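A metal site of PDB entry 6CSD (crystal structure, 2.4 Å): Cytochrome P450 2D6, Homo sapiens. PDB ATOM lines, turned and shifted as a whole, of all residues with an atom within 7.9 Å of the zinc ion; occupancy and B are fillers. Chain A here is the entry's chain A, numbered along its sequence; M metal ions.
ND1 of His 236 sits close to O of Cys 169 (3.4 Å).
O of His 236 lies within hydrogen-bond range of OG1 of Thr 239, 3.3 Å away.
OE2 of Glu 251 sits at hydrogen-bond distance from N of Arg 247.
The side-chain carboxylate of Asp 248 sits at hydrogen-bond distance from the backbone NH of Thr 250 (3.3 Å).
The zinc ion is bound by a ring nitrogen (NE2) of His 236 (1.9 Å), the side-chain carboxylate (OE1) of Glu 251 (1.9 Å) and the side-chain carboxylate (OD2) of Asp 248 (2.0 Å).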
ATOM      1  N   SER A 166     -25.404 -25.032  36.128  1.00  0.00           N
ATOM      2  CA  SER A 166     -25.809 -24.408  34.881  1.00  0.00           C
ATOM      3  C   SER A 166     -25.008 -23.146  34.603  1.00  0.00           C
ATOM      4  O   SER A 166     -24.599 -22.916  33.449  1.00  0.00           O
ATOM      5  CB  SER A 166     -27.301 -24.099  34.904  1.00  0.00           C
ATOM      6  OG  SER A 166     -27.665 -23.495  33.682  1.00  0.00           O
ATOM      7  N   LEU A 167     -24.785 -22.315  35.633  1.00  0.00           N
ATOM      8  CA  LEU A 167     -24.069 -21.052  35.474  1.00  0.00           C
ATOM      9  C   LEU A 167     -22.575 -21.271  35.236  1.00  0.00           C
ATOM     10  O   LEU A 167     -21.984 -20.582  34.418  1.00  0.00           O
ATOM     11  CB  LEU A 167     -24.269 -20.146  36.708  1.00  0.00           C
ATOM     12  CG  LEU A 167     -25.684 -19.553  36.905  1.00  0.00           C
ATOM     13  CD1 LEU A 167     -25.980 -19.238  38.367  1.00  0.00           C
ATOM     14  CD2 LEU A 167     -25.901 -18.316  36.033  1.00  0.00           C
ATOM     15  N   THR A 168     -21.968 -22.206  35.949  1.00  0.00           N
ATOM     16  CA  THR A 168     -20.541 -22.427  35.803  1.00  0.00           C
ATOM     17  C   THR A 168     -20.185 -23.385  34.676  1.00  0.00           C
ATOM     18  O   THR A 168     -19.224 -23.148  33.930  1.00  0.00           O
ATOM     19  CB  THR A 168     -19.963 -22.975  37.100  1.00  0.00           C
ATOM     20  OG1 THR A 168     -20.669 -24.172  37.451  1.00  0.00           O
ATOM     21  CG2 THR A 168     -20.107 -21.961  38.225  1.00  0.00           C
ATOM     22  N   CYS A 169     -20.951 -24.466  34.502  1.00  0.00           N
ATOM     23  CA  CYS A 169     -20.563 -25.529  33.612  1.00  0.00           C
ATOM     24  C   CYS A 169     -21.479 -25.661  32.403  1.00  0.00           C
ATOM     25  O   CYS A 169     -21.205 -26.489  31.547  1.00  0.00           O
ATOM     26  CB  CYS A 169     -20.492 -26.834  34.402  1.00  0.00           C
ATOM     27  SG  CYS A 169     -19.065 -26.858  35.506  1.00  0.00           S
ATOM     28  N   GLY A 170     -22.508 -24.838  32.294  1.00  0.00           N
ATOM     29  CA  GLY A 170     -23.356 -24.839  31.112  1.00  0.00           C
ATOM     30  C   GLY A 170     -24.215 -26.074  30.986  1.00  0.00           C
ATOM     31  O   GLY A 170     -24.652 -26.395  29.872  1.00  0.00           O
ATOM     32  N   ARG A 171     -24.480 -26.785  32.072  1.00  0.00           N
ATOM     33  CA  ARG A 171     -25.281 -27.992  31.980  1.00  0.00           C
ATOM     34  C   ARG A 171     -25.879 -28.312  33.355  1.00  0.00           C
ATOM     35  O   ARG A 171     -25.378 -27.874  34.397  1.00  0.00           O
ATOM     36  CB  ARG A 171     -24.425 -29.154  31.500  1.00  0.00           C
ATOM     37  CG  ARG A 171     -23.445 -29.607  32.548  1.00  0.00           C
ATOM     38  CD  ARG A 171     -22.939 -30.990  32.313  1.00  0.00           C
ATOM     39  NE  ARG A 171     -23.992 -32.010  32.360  1.00  0.00           N
ATOM     40  CZ  ARG A 171     -23.826 -33.289  32.042  1.00  0.00           C
ATOM     41  NH1 ARG A 171     -22.637 -33.729  31.659  1.00  0.00           N
ATOM     42  NH2 ARG A 171     -24.855 -34.137  32.146  1.00  0.00           N
ATOM     43  N   HIS A 236     -15.960 -30.178  28.874  1.00  0.00           N
ATOM     44  CA  HIS A 236     -16.427 -28.838  28.520  1.00  0.00           C
ATOM     45  C   HIS A 236     -15.489 -28.176  27.528  1.00  0.00           C
ATOM     46  O   HIS A 236     -15.934 -27.477  26.617  1.00  0.00           O
ATOM     47  CB  HIS A 236     -16.569 -27.977  29.792  1.00  0.00           C
ATOM     48  CG  HIS A 236     -17.514 -26.829  29.638  1.00  0.00           C
ATOM     49  ND1 HIS A 236     -17.925 -26.057  30.695  1.00  0.00           N
ATOM     50  CD2 HIS A 236     -18.133 -26.321  28.547  1.00  0.00           C
ATOM     51  CE1 HIS A 236     -18.765 -25.122  30.259  1.00  0.00           C
ATOM     52  NE2 HIS A 236     -18.911 -25.279  28.959  1.00  0.00           N
ATOM     53  N   ARG A 237     -14.173 -28.382  27.696  1.00  0.00           N
ATOM     54  CA  ARG A 237     -13.201 -27.857  26.736  1.00  0.00           C
ATOM     55  C   ARG A 237     -13.421 -28.452  25.366  1.00  0.00           C
ATOM     56  O   ARG A 237     -13.255 -27.764  24.348  1.00  0.00           O
ATOM     57  CB  ARG A 237     -11.777 -28.151  27.214  1.00  0.00           C
ATOM     58  CG  ARG A 237     -11.209 -27.167  28.226  1.00  0.00           C
ATOM     59  CD  ARG A 237      -9.675 -27.286  28.322  1.00  0.00           C
ATOM     60  NE  ARG A 237      -9.227 -27.358  29.713  1.00  0.00           N
ATOM     61  CZ  ARG A 237      -8.339 -26.535  30.260  1.00  0.00           C
ATOM     62  NH1 ARG A 237      -7.786 -25.558  29.553  1.00  0.00           N
ATOM     63  NH2 ARG A 237      -7.999 -26.688  31.539  1.00  0.00           N
ATOM     64  N   THR A 239     -16.411 -29.404  24.156  1.00  0.00           N
ATOM     65  CA  THR A 239     -17.666 -28.940  23.585  1.00  0.00           C
ATOM     66  C   THR A 239     -17.757 -27.428  23.440  1.00  0.00           C
ATOM     67  O   THR A 239     -18.716 -26.924  22.844  1.00  0.00           O
ATOM     68  CB  THR A 239     -18.864 -29.435  24.411  1.00  0.00           C
ATOM     69  OG1 THR A 239     -18.836 -28.812  25.702  1.00  0.00           O
ATOM     70  CG2 THR A 239     -18.785 -30.929  24.596  1.00  0.00           C
ATOM     71  N   TRP A 240     -16.802 -26.691  23.983  1.00  0.00           N
ATOM     72  CA  TRP A 240     -16.842 -25.234  23.958  1.00  0.00           C
ATOM     73  C   TRP A 240     -16.699 -24.729  22.529  1.00  0.00           C
ATOM     74  O   TRP A 240     -15.871 -25.233  21.759  1.00  0.00           O
ATOM     75  CB  TRP A 240     -15.736 -24.677  24.871  1.00  0.00           C
ATOM     76  CG  TRP A 240     -15.441 -23.207  24.758  1.00  0.00           C
ATOM     77  CD1 TRP A 240     -16.340 -22.193  24.565  1.00  0.00           C
ATOM     78  CD2 TRP A 240     -14.160 -22.586  24.832  1.00  0.00           C
ATOM     79  NE1 TRP A 240     -15.703 -21.001  24.509  1.00  0.00           N
ATOM     80  CE2 TRP A 240     -14.350 -21.206  24.680  1.00  0.00           C
ATOM     81  CE3 TRP A 240     -12.852 -23.070  25.024  1.00  0.00           C
ATOM     82  CZ2 TRP A 240     -13.285 -20.279  24.714  1.00  0.00           C
ATOM     83  CZ3 TRP A 240     -11.792 -22.151  25.055  1.00  0.00           C
ATOM     84  CH2 TRP A 240     -12.021 -20.780  24.888  1.00  0.00           C
ATOM     85  N   ASP A 241     -17.537 -23.764  22.150  1.00  0.00           N
ATOM     86  CA  ASP A 241     -17.461 -23.116  20.849  1.00  0.00           C
ATOM     87  C   ASP A 241     -16.962 -21.689  21.031  1.00  0.00           C
ATOM     88  O   ASP A 241     -17.779 -20.776  21.202  1.00  0.00           O
ATOM     89  CB  ASP A 241     -18.834 -23.120  20.157  1.00  0.00           C
ATOM     90  CG  ASP A 241     -18.763 -22.638  18.710  1.00  0.00           C
ATOM     91  OD1 ASP A 241     -17.667 -22.207  18.279  1.00  0.00           O
ATOM     92  OD2 ASP A 241     -19.791 -22.672  18.004  1.00  0.00           O
ATOM     93  N   PRO A 245     -20.364 -16.299  21.842  1.00  0.00           N
ATOM     94  CA  PRO A 245     -20.183 -15.691  23.167  1.00  0.00           C
ATOM     95  C   PRO A 245     -20.276 -16.733  24.264  1.00  0.00           C
ATOM     96  O   PRO A 245     -21.030 -17.711  24.158  1.00  0.00           O
ATOM     97  CB  PRO A 245     -21.348 -14.684  23.261  1.00  0.00           C
ATOM     98  CG  PRO A 245     -21.737 -14.402  21.816  1.00  0.00           C
ATOM     99  CD  PRO A 245     -21.435 -15.660  21.057  1.00  0.00           C
ATOM    100  N   PRO A 246     -19.529 -16.551  25.361  1.00  0.00           N
ATOM    101  CA  PRO A 246     -19.544 -17.560  26.436  1.00  0.00           C
ATOM    102  C   PRO A 246     -20.957 -17.841  26.935  1.00  0.00           C
ATOM    103  O   PRO A 246     -21.724 -16.917  27.211  1.00  0.00           O
ATOM    104  CB  PRO A 246     -18.666 -16.919  27.509  1.00  0.00           C
ATOM    105  CG  PRO A 246     -17.758 -15.976  26.747  1.00  0.00           C
ATOM    106  CD  PRO A 246     -18.653 -15.402  25.689  1.00  0.00           C
ATOM    107  N   ARG A 247     -21.312 -19.128  27.001  1.00  0.00           N
ATOM    108  CA  ARG A 247     -22.593 -19.560  27.545  1.00  0.00           C
ATOM    109  C   ARG A 247     -22.593 -19.670  29.055  1.00  0.00           C
ATOM    110  O   ARG A 247     -23.660 -19.698  29.674  1.00  0.00           O
ATOM    111  CB  ARG A 247     -22.965 -20.924  26.965  1.00  0.00           C
ATOM    112  CG  ARG A 247     -23.582 -20.877  25.585  1.00  0.00           C
ATOM    113  CD  ARG A 247     -24.538 -22.039  25.408  1.00  0.00           C
ATOM    114  NE  ARG A 247     -24.212 -23.063  26.394  1.00  0.00           N
ATOM    115  CZ  ARG A 247     -25.039 -23.561  27.303  1.00  0.00           C
ATOM    116  NH1 ARG A 247     -26.294 -23.140  27.371  1.00  0.00           N
ATOM    117  NH2 ARG A 247     -24.592 -24.468  28.152  1.00  0.00           N
ATOM    118  N   ASP A 248     -21.421 -19.777  29.671  1.00  0.00           N
ATOM    119  CA  ASP A 248     -21.340 -20.085  31.085  1.00  0.00           C
ATOM    120  C   ASP A 248     -20.023 -19.548  31.593  1.00  0.00           C
ATOM    121  O   ASP A 248     -19.180 -19.091  30.825  1.00  0.00           O
ATOM    122  CB  ASP A 248     -21.434 -21.590  31.323  1.00  0.00           C
ATOM    123  CG  ASP A 248     -20.504 -22.360  30.405  1.00  0.00           C
ATOM    124  OD1 ASP A 248     -19.264 -22.308  30.580  1.00  0.00           O
ATOM    125  OD2 ASP A 248     -21.021 -22.962  29.460  1.00  0.00           O
ATOM    126  N   LEU A 249     -19.842 -19.665  32.901  1.00  0.00           N
ATOM    127  CA  LEU A 249     -18.702 -19.024  33.525  1.00  0.00           C
ATOM    128  C   LEU A 249     -17.385 -19.689  33.124  1.00  0.00           C
ATOM    129  O   LEU A 249     -16.367 -19.010  32.967  1.00  0.00           O
ATOM    130  CB  LEU A 249     -18.902 -19.014  35.058  1.00  0.00           C
ATOM    131  CG  LEU A 249     -17.736 -18.369  35.809  1.00  0.00           C
ATOM    132  CD1 LEU A 249     -18.245 -17.366  36.884  1.00  0.00           C
ATOM    133  CD2 LEU A 249     -16.877 -19.462  36.407  1.00  0.00           C
ATOM    134  N   THR A 250     -17.378 -21.014  32.978  1.00  0.00           N
ATOM    135  CA  THR A 250     -16.165 -21.694  32.516  1.00  0.00           C
ATOM    136  C   THR A 250     -15.731 -21.195  31.140  1.00  0.00           C
ATOM    137  O   THR A 250     -14.533 -21.032  30.882  1.00  0.00           O
ATOM    138  CB  THR A 250     -16.400 -23.200  32.520  1.00  0.00           C
ATOM    139  OG1 THR A 250     -16.454 -23.641  33.881  1.00  0.00           O
ATOM    140  CG2 THR A 250     -15.270 -23.969  31.804  1.00  0.00           C
ATOM    141  N   GLU A 251     -16.692 -20.928  30.232  1.00  0.00           N
ATOM    142  CA  GLU A 251     -16.296 -20.459  28.913  1.00  0.00           C
ATOM    143  C   GLU A 251     -15.769 -19.047  29.009  1.00  0.00           C
ATOM    144  O   GLU A 251     -14.747 -18.703  28.382  1.00  0.00           O
ATOM    145  CB  GLU A 251     -17.470 -20.552  27.902  1.00  0.00           C
ATOM    146  CG  GLU A 251     -17.891 -21.966  27.535  1.00  0.00           C
ATOM    147  CD  GLU A 251     -19.129 -21.988  26.646  1.00  0.00           C
ATOM    148  OE1 GLU A 251     -19.844 -23.009  26.604  1.00  0.00           O
ATOM    149  OE2 GLU A 251     -19.416 -20.951  26.008  1.00  0.00           O
ATOM    150  N   ALA A 252     -16.437 -18.215  29.816  1.00  0.00           N
ATOM    151  CA  ALA A 252     -15.916 -16.864  30.043  1.00  0.00           C
ATOM    152  C   ALA A 252     -14.500 -16.921  30.583  1.00  0.00           C
ATOM    153  O   ALA A 252     -13.620 -16.162  30.158  1.00  0.00           O
ATOM    154  CB  ALA A 252     -16.853 -16.096  30.979  1.00  0.00           C
ATOM    155  N   LEU A 254     -12.255 -19.403  30.170  1.00  0.00           N
ATOM    156  CA  LEU A 254     -11.335 -19.920  29.155  1.00  0.00           C
ATOM    157  C   LEU A 254     -11.000 -18.838  28.130  1.00  0.00           C
ATOM    158  O   LEU A 254      -9.835 -18.710  27.739  1.00  0.00           O
ATOM    159  CB  LEU A 254     -11.935 -21.147  28.482  1.00  0.00           C
ATOM    160  CG  LEU A 254     -12.119 -22.446  29.264  1.00  0.00           C
ATOM    161  CD1 LEU A 254     -13.144 -23.306  28.555  1.00  0.00           C
ATOM    162  CD2 LEU A 254     -10.836 -23.227  29.493  1.00  0.00           C
HETATM  163 ZN    ZN M   1     -20.168 -24.188  28.073  1.00  0.00          ZN
